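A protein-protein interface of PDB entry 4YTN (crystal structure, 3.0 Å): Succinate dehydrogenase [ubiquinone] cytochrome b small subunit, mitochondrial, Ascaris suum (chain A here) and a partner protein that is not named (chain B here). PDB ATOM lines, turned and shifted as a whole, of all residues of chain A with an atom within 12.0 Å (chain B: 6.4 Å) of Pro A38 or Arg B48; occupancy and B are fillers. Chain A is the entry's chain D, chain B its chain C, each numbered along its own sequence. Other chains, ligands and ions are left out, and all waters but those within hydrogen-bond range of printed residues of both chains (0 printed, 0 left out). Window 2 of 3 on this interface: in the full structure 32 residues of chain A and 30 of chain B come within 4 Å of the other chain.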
ATOM      1  N   GLY A  34     -15.169   8.600   6.575  1.00  0.00           N
ATOM      2  CA  GLY A  34     -14.870   8.905   7.972  1.00  0.00           C
ATOM      3  C   GLY A  34     -13.459   9.403   8.162  1.00  0.00           C
ATOM      4  O   GLY A  34     -12.628   9.287   7.265  1.00  0.00           O
ATOM      5  N   ALA A  35     -13.202   9.957   9.345  1.00  0.00           N
ATOM      6  CA  ALA A  35     -11.910  10.548   9.675  1.00  0.00           C
ATOM      7  C   ALA A  35     -11.093   9.585  10.529  1.00  0.00           C
ATOM      8  O   ALA A  35     -11.618   8.596  11.047  1.00  0.00           O
ATOM      9  CB  ALA A  35     -12.109  11.868  10.407  1.00  0.00           C
ATOM     10  N   ALA A  36      -9.805   9.881  10.676  1.00  0.00           N
ATOM     11  CA  ALA A  36      -8.926   9.082  11.529  1.00  0.00           C
ATOM     12  C   ALA A  36      -9.402   9.185  12.965  1.00  0.00           C
ATOM     13  O   ALA A  36      -9.927  10.222  13.372  1.00  0.00           O
ATOM     14  CB  ALA A  36      -7.478   9.554  11.427  1.00  0.00           C
ATOM     15  N   PRO A  37      -9.229   8.107  13.742  1.00  0.00           N
ATOM     16  CA  PRO A  37      -9.580   8.205  15.148  1.00  0.00           C
ATOM     17  C   PRO A  37      -8.705   9.246  15.862  1.00  0.00           C
ATOM     18  O   PRO A  37      -7.621   9.575  15.372  1.00  0.00           O
ATOM     19  CB  PRO A  37      -9.312   6.791  15.673  1.00  0.00           C
ATOM     20  CG  PRO A  37      -8.258   6.263  14.766  1.00  0.00           C
ATOM     21  CD  PRO A  37      -8.626   6.804  13.418  1.00  0.00           C
ATOM     22  N   PRO A  38      -9.179   9.773  17.004  1.00  0.00           N
ATOM     23  CA  PRO A  38      -8.384  10.740  17.733  1.00  0.00           C
ATOM     24  C   PRO A  38      -7.180  10.050  18.330  1.00  0.00           C
ATOM     25  O   PRO A  38      -7.305   8.984  18.934  1.00  0.00           O
ATOM     26  CB  PRO A  38      -9.332  11.235  18.822  1.00  0.00           C
ATOM     27  CG  PRO A  38     -10.277  10.119  19.041  1.00  0.00           C
ATOM     28  CD  PRO A  38     -10.404   9.399  17.733  1.00  0.00           C
ATOM     29  N   GLN A  39      -6.026  10.672  18.146  1.00  0.00           N
ATOM     30  CA  GLN A  39      -4.747  10.053  18.428  1.00  0.00           C
ATOM     31  C   GLN A  39      -3.747  11.159  18.707  1.00  0.00           C
ATOM     32  O   GLN A  39      -3.823  12.239  18.116  1.00  0.00           O
ATOM     33  CB  GLN A  39      -4.324   9.217  17.214  1.00  0.00           C
ATOM     34  CG  GLN A  39      -2.853   8.818  17.164  1.00  0.00           C
ATOM     35  CD  GLN A  39      -2.598   7.640  16.242  1.00  0.00           C
ATOM     36  OE1 GLN A  39      -3.449   6.766  16.084  1.00  0.00           O
ATOM     37  NE2 GLN A  39      -1.420   7.602  15.642  1.00  0.00           N
ATOM     38  N   PHE A  40      -2.819  10.900  19.612  1.00  0.00           N
ATOM     39  CA  PHE A  40      -1.861  11.913  20.005  1.00  0.00           C
ATOM     40  C   PHE A  40      -0.596  11.720  19.220  1.00  0.00           C
ATOM     41  O   PHE A  40       0.034  10.678  19.315  1.00  0.00           O
ATOM     42  CB  PHE A  40      -1.562  11.821  21.495  1.00  0.00           C
ATOM     43  CG  PHE A  40      -0.690  12.924  21.996  1.00  0.00           C
ATOM     44  CD1 PHE A  40      -1.203  14.193  22.185  1.00  0.00           C
ATOM     45  CD2 PHE A  40       0.651  12.696  22.280  1.00  0.00           C
ATOM     46  CE1 PHE A  40      -0.400  15.219  22.651  1.00  0.00           C
ATOM     47  CE2 PHE A  40       1.459  13.717  22.751  1.00  0.00           C
ATOM     48  CZ  PHE A  40       0.933  14.983  22.934  1.00  0.00           C
ATOM     49  N   ASP A  41      -0.230  12.722  18.433  1.00  0.00           N
ATOM     50  CA  ASP A  41       1.027  12.704  17.698  1.00  0.00           C
ATOM     51  C   ASP A  41       2.070  13.423  18.534  1.00  0.00           C
ATOM     52  O   ASP A  41       2.054  14.649  18.604  1.00  0.00           O
ATOM     53  CB  ASP A  41       0.855  13.399  16.353  1.00  0.00           C
ATOM     54  CG  ASP A  41       2.108  13.363  15.507  1.00  0.00           C
ATOM     55  OD1 ASP A  41       3.173  12.911  15.995  1.00  0.00           O
ATOM     56  OD2 ASP A  41       2.018  13.797  14.337  1.00  0.00           O
ATOM     57  N   PRO A  42       2.990  12.669  19.165  1.00  0.00           N
ATOM     58  CA  PRO A  42       3.947  13.293  20.072  1.00  0.00           C
ATOM     59  C   PRO A  42       5.047  14.091  19.364  1.00  0.00           C
ATOM     60  O   PRO A  42       5.751  14.852  20.022  1.00  0.00           O
ATOM     61  CB  PRO A  42       4.543  12.100  20.815  1.00  0.00           C
ATOM     62  CG  PRO A  42       4.491  10.995  19.822  1.00  0.00           C
ATOM     63  CD  PRO A  42       3.298  11.245  18.942  1.00  0.00           C
ATOM     64  N   ALA A  44       4.244  15.943  16.356  1.00  0.00           N
ATOM     65  CA  ALA A  44       3.484  17.148  15.993  1.00  0.00           C
ATOM     66  C   ALA A  44       3.313  18.085  17.191  1.00  0.00           C
ATOM     67  O   ALA A  44       3.215  19.299  17.025  1.00  0.00           O
ATOM     68  CB  ALA A  44       2.120  16.777  15.415  1.00  0.00           C
ATOM     69  N   PHE A 111     -13.310  20.128  35.301  1.00  0.00           N
ATOM     70  CA  PHE A 111     -14.221  19.073  34.834  1.00  0.00           C
ATOM     71  C   PHE A 111     -15.448  18.967  35.724  1.00  0.00           C
ATOM     72  O   PHE A 111     -16.554  18.815  35.225  1.00  0.00           O
ATOM     73  CB  PHE A 111     -13.524  17.707  34.761  1.00  0.00           C
ATOM     74  CG  PHE A 111     -14.405  16.592  34.232  1.00  0.00           C
ATOM     75  CD1 PHE A 111     -14.527  16.369  32.859  1.00  0.00           C
ATOM     76  CD2 PHE A 111     -15.105  15.755  35.107  1.00  0.00           C
ATOM     77  CE1 PHE A 111     -15.332  15.348  32.369  1.00  0.00           C
ATOM     78  CE2 PHE A 111     -15.912  14.727  34.622  1.00  0.00           C
ATOM     79  CZ  PHE A 111     -16.028  14.527  33.252  1.00  0.00           C
ATOM     80  N   TRP B  41      -4.717  17.717  24.930  1.00  0.00           N
ATOM     81  CA  TRP B  41      -5.313  16.507  24.376  1.00  0.00           C
ATOM     82  C   TRP B  41      -6.159  15.802  25.435  1.00  0.00           C
ATOM     83  O   TRP B  41      -7.300  15.414  25.180  1.00  0.00           O
ATOM     84  CB  TRP B  41      -4.225  15.561  23.848  1.00  0.00           C
ATOM     85  CG  TRP B  41      -4.759  14.447  23.000  1.00  0.00           C
ATOM     86  CD1 TRP B  41      -4.822  14.416  21.645  1.00  0.00           C
ATOM     87  CD2 TRP B  41      -5.310  13.201  23.459  1.00  0.00           C
ATOM     88  NE1 TRP B  41      -5.375  13.231  21.222  1.00  0.00           N
ATOM     89  CE2 TRP B  41      -5.685  12.469  22.318  1.00  0.00           C
ATOM     90  CE3 TRP B  41      -5.518  12.632  24.725  1.00  0.00           C
ATOM     91  CZ2 TRP B  41      -6.259  11.199  22.399  1.00  0.00           C
ATOM     92  CZ3 TRP B  41      -6.090  11.371  24.804  1.00  0.00           C
ATOM     93  CH2 TRP B  41      -6.457  10.671  23.650  1.00  0.00           C
ATOM     94  N   GLY B  42      -5.595  15.649  26.625  1.00  0.00           N
ATOM     95  CA  GLY B  42      -6.302  15.018  27.726  1.00  0.00           C
ATOM     96  C   GLY B  42      -7.616  15.699  28.057  1.00  0.00           C
ATOM     97  O   GLY B  42      -8.584  15.030  28.438  1.00  0.00           O
ATOM     98  N   TRP B  43      -7.658  17.024  27.917  1.00  0.00           N
ATOM     99  CA  TRP B  43      -8.863  17.751  28.260  1.00  0.00           C
ATOM    100  C   TRP B  43      -9.965  17.400  27.276  1.00  0.00           C
ATOM    101  O   TRP B  43     -11.083  17.069  27.677  1.00  0.00           O
ATOM    102  CB  TRP B  43      -8.649  19.267  28.297  1.00  0.00           C
ATOM    103  CG  TRP B  43      -9.954  19.977  28.480  1.00  0.00           C
ATOM    104  CD1 TRP B  43     -10.727  20.549  27.503  1.00  0.00           C
ATOM    105  CD2 TRP B  43     -10.676  20.125  29.700  1.00  0.00           C
ATOM    106  NE1 TRP B  43     -11.873  21.061  28.050  1.00  0.00           N
ATOM    107  CE2 TRP B  43     -11.872  20.811  29.398  1.00  0.00           C
ATOM    108  CE3 TRP B  43     -10.432  19.747  31.022  1.00  0.00           C
ATOM    109  CZ2 TRP B  43     -12.817  21.135  30.375  1.00  0.00           C
ATOM    110  CZ3 TRP B  43     -11.379  20.060  31.996  1.00  0.00           C
ATOM    111  CH2 TRP B  43     -12.552  20.752  31.666  1.00  0.00           C
ATOM    112  N   ASP B  44      -9.639  17.471  25.990  1.00  0.00           N
ATOM    113  CA  ASP B  44     -10.587  17.130  24.934  1.00  0.00           C
ATOM    114  C   ASP B  44     -11.109  15.709  25.130  1.00  0.00           C
ATOM    115  O   ASP B  44     -12.308  15.445  24.956  1.00  0.00           O
ATOM    116  CB  ASP B  44      -9.925  17.273  23.564  1.00  0.00           C
ATOM    117  CG  ASP B  44      -9.550  18.709  23.248  1.00  0.00           C
ATOM    118  OD1 ASP B  44      -8.544  18.918  22.544  1.00  0.00           O
ATOM    119  OD2 ASP B  44     -10.251  19.631  23.708  1.00  0.00           O
ATOM    120  N   TYR B  45     -10.205  14.810  25.516  1.00  0.00           N
ATOM    121  CA  TYR B  45     -10.568  13.433  25.813  1.00  0.00           C
ATOM    122  C   TYR B  45     -11.712  13.388  26.817  1.00  0.00           C
ATOM    123  O   TYR B  45     -12.759  12.777  26.557  1.00  0.00           O
ATOM    124  CB  TYR B  45      -9.371  12.641  26.358  1.00  0.00           C
ATOM    125  CG  TYR B  45      -9.774  11.289  26.898  1.00  0.00           C
ATOM    126  CD1 TYR B  45     -10.070  10.232  26.038  1.00  0.00           C
ATOM    127  CD2 TYR B  45      -9.902  11.079  28.265  1.00  0.00           C
ATOM    128  CE1 TYR B  45     -10.463   8.997  26.529  1.00  0.00           C
ATOM    129  CE2 TYR B  45     -10.291   9.850  28.764  1.00  0.00           C
ATOM    130  CZ  TYR B  45     -10.568   8.811  27.897  1.00  0.00           C
ATOM    131  OH  TYR B  45     -10.949   7.590  28.420  1.00  0.00           O
ATOM    132  N   LEU B  46     -11.504  14.034  27.960  1.00  0.00           N
ATOM    133  CA  LEU B  46     -12.517  14.066  29.004  1.00  0.00           C
ATOM    134  C   LEU B  46     -13.839  14.626  28.476  1.00  0.00           C
ATOM    135  O   LEU B  46     -14.915  14.163  28.864  1.00  0.00           O
ATOM    136  CB  LEU B  46     -12.041  14.876  30.213  1.00  0.00           C
ATOM    137  CG  LEU B  46     -10.825  14.364  31.005  1.00  0.00           C
ATOM    138  CD1 LEU B  46     -10.575  15.294  32.184  1.00  0.00           C
ATOM    139  CD2 LEU B  46     -10.991  12.934  31.494  1.00  0.00           C
ATOM    140  N   MET B  47     -13.760  15.602  27.577  1.00  0.00           N
ATOM    141  CA  MET B  47     -14.960  16.211  27.020  1.00  0.00           C
ATOM    142  C   MET B  47     -15.671  15.239  26.091  1.00  0.00           C
ATOM    143  O   MET B  47     -16.877  15.019  26.221  1.00  0.00           O
ATOM    144  CB  MET B  47     -14.615  17.506  26.294  1.00  0.00           C
ATOM    145  CG  MET B  47     -14.020  18.571  27.206  1.00  0.00           C
ATOM    146  SD  MET B  47     -15.152  19.234  28.444  1.00  0.00           S
ATOM    147  CE  MET B  47     -14.859  18.202  29.868  1.00  0.00           C
ATOM    148  N   ARG B  48     -14.920  14.651  25.165  1.00  0.00           N
ATOM    149  CA  ARG B  48     -15.441  13.559  24.338  1.00  0.00           C
ATOM    150  C   ARG B  48     -16.178  12.501  25.170  1.00  0.00           C
ATOM    151  O   ARG B  48     -17.195  11.951  24.743  1.00  0.00           O
ATOM    152  CB  ARG B  48     -14.301  12.867  23.604  1.00  0.00           C
ATOM    153  CG  ARG B  48     -14.180  13.185  22.137  1.00  0.00           C
ATOM    154  CD  ARG B  48     -12.896  12.566  21.624  1.00  0.00           C
ATOM    155  NE  ARG B  48     -11.738  13.339  22.057  1.00  0.00           N
ATOM    156  CZ  ARG B  48     -10.498  12.868  22.163  1.00  0.00           C
ATOM    157  NH1 ARG B  48     -10.226  11.597  21.876  1.00  0.00           N
ATOM    158  NH2 ARG B  48      -9.517  13.677  22.568  1.00  0.00           N
ATOM    159  N   GLN B  49     -15.634  12.203  26.347  1.00  0.00           N
ATOM    160  CA  GLN B  49     -16.178  11.172  27.203  1.00  0.00           C
ATOM    161  C   GLN B  49     -17.473  11.628  27.824  1.00  0.00           C
ATOM    162  O   GLN B  49     -18.432  10.858  27.892  1.00  0.00           O
ATOM    163  CB  GLN B  49     -15.166  10.791  28.283  1.00  0.00           C
ATOM    164  CG  GLN B  49     -13.947  10.075  27.724  1.00  0.00           C
ATOM    165  CD  GLN B  49     -14.299   8.706  27.205  1.00  0.00           C
ATOM    166  OE1 GLN B  49     -14.834   7.891  27.930  1.00  0.00           O
ATOM    167  NE2 GLN B  49     -14.022   8.457  25.940  1.00  0.00           N
ATOM    168  N   ARG B  50     -17.511  12.880  28.272  1.00  0.00           N
ATOM    169  CA  ARG B  50     -18.762  13.456  28.758  1.00  0.00           C
ATOM    170  C   ARG B  50     -19.831  13.368  27.674  1.00  0.00           C
ATOM    171  O   ARG B  50     -20.961  12.951  27.937  1.00  0.00           O
ATOM    172  CB  ARG B  50     -18.580  14.912  29.181  1.00  0.00           C
ATOM    173  CG  ARG B  50     -19.890  15.599  29.548  1.00  0.00           C
ATOM    174  CD  ARG B  50     -19.652  16.937  30.223  1.00  0.00           C
ATOM    175  NE  ARG B  50     -19.068  16.767  31.554  1.00  0.00           N
ATOM    176  CZ  ARG B  50     -18.326  17.677  32.185  1.00  0.00           C
ATOM    177  NH1 ARG B  50     -18.055  18.856  31.625  1.00  0.00           N
ATOM    178  NH2 ARG B  50     -17.844  17.399  33.389  1.00  0.00           N
ATOM    179  N   ALA B  51     -19.454  13.754  26.456  1.00  0.00           N
ATOM    180  CA  ALA B  51     -20.349  13.699  25.299  1.00  0.00           C
ATOM    181  C   ALA B  51     -21.002  12.325  25.140  1.00  0.00           C
ATOM    182  O   ALA B  51     -22.207  12.229  24.923  1.00  0.00           O
ATOM    183  CB  ALA B  51     -19.592  14.069  24.030  1.00  0.00           C
ATOM    184  N   LEU B  52     -20.200  11.270  25.274  1.00  0.00           N
ATOM    185  CA  LEU B  52     -20.686   9.895  25.149  1.00  0.00           C
ATOM    186  C   LEU B  52     -21.463   9.380  26.375  1.00  0.00           C
ATOM    187  O   LEU B  52     -21.806   8.199  26.431  1.00  0.00           O
ATOM    188  CB  LEU B  52     -19.514   8.948  24.845  1.00  0.00           C
ATOM    189  CG  LEU B  52     -18.791   9.123  23.502  1.00  0.00           C
ATOM    190  CD1 LEU B  52     -17.519   8.297  23.491  1.00  0.00           C
ATOM    191  CD2 LEU B  52     -19.666   8.735  22.321  1.00  0.00           C
ATOM    192  N   LYS B  53     -21.733  10.247  27.351  1.00  0.00           N
ATOM    193  CA  LYS B  53     -22.544   9.885  28.521  1.00  0.00           C
ATOM    194  C   LYS B  53     -22.054   8.618  29.238  1.00  0.00           C
ATOM    195  O   LYS B  53     -22.855   7.876  29.803  1.00  0.00           O
ATOM    196  CB  LYS B  53     -24.027   9.713  28.120  1.00  0.00           C
ATOM    197  CG  LYS B  53     -24.877  10.977  28.190  1.00  0.00           C
ATOM    198  CD  LYS B  53     -24.669  11.860  26.974  1.00  0.00           C
ATOM    199  CE  LYS B  53     -25.099  13.291  27.244  1.00  0.00           C
ATOM    200  NZ  LYS B  53     -26.544  13.380  27.593  1.00  0.00           N
ATOM    201  N   ARG B  54     -20.750   8.367  29.221  1.00  0.00           N
ATOM    202  CA  ARG B  54     -20.221   7.142  29.820  1.00  0.00           C
ATOM    203  C   ARG B  54     -20.064   7.294  31.321  1.00  0.00           C
ATOM    204  O   ARG B  54     -19.592   8.321  31.793  1.00  0.00           O
ATOM    205  CB  ARG B  54     -18.869   6.788  29.222  1.00  0.00           C
ATOM    206  CG  ARG B  54     -18.957   6.339  27.789  1.00  0.00           C
ATOM    207  CD  ARG B  54     -17.584   6.196  27.175  1.00  0.00           C
ATOM    208  NE  ARG B  54     -17.664   5.452  25.927  1.00  0.00           N
ATOM    209  CZ  ARG B  54     -16.666   5.302  25.069  1.00  0.00           C
ATOM    210  NH1 ARG B  54     -15.482   5.854  25.296  1.00  0.00           N
ATOM    211  NH2 ARG B  54     -16.862   4.599  23.966  1.00  0.00           N
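The indole nitrogen (NE1) of Trp B43 lies close to the side-chain sulfur (SD) of Met B47, 3.8 Å away.
O of Phe A111 lies within hydrogen-bond range of NH2 of Arg B50 (2.7 Å).
Of chain B, only Arg B48 (3.2 Å) comes within 4 Å of Pro A38. Arg B48 touches one residue of chain A. Of the printed residues of chain A, Trp B41 touches Gln A39 (3.6 Å) and Phe A40 (3.7 Å). No residue of chain A comes within 4 Å of Asp B44. Tyr B45 touches none of the printed residues of chain A. Of chain A, only Phe A111 comes within 4 Å of Met B47. No residue of chain A comes within 4 Å of Ala B51. Leu B52 touches none of the printed residues of chain A. Of the printed residues of chain A, Trp B43 touches Phe A111 (3.8 Å). Printed residues of chain A within 4 Å of Arg B50: Phe A111. Ala A35 touches none of the printed residues of chain B. Pro A42 touches none of the printed residues of chain B.
Among the printed residues, pairs that only touch across the chains: Pro A38 with Arg B48, Phe A111 with Met B47, Gln A39 with Trp B41, Phe A40 with Trp B41, Phe A111 with Leu B46 and Phe A111 with Trp B43.
Of the 14 printed residues of chain B, 6 touch a printed residue of chain A. Along chain A the printed residues that touch a printed residue of chain B span positions 38 to 111. Among the printed residues, no Asp or Glu carboxylate lies within 4 Å of a Lys or Arg side-chain nitrogen of the other chain.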
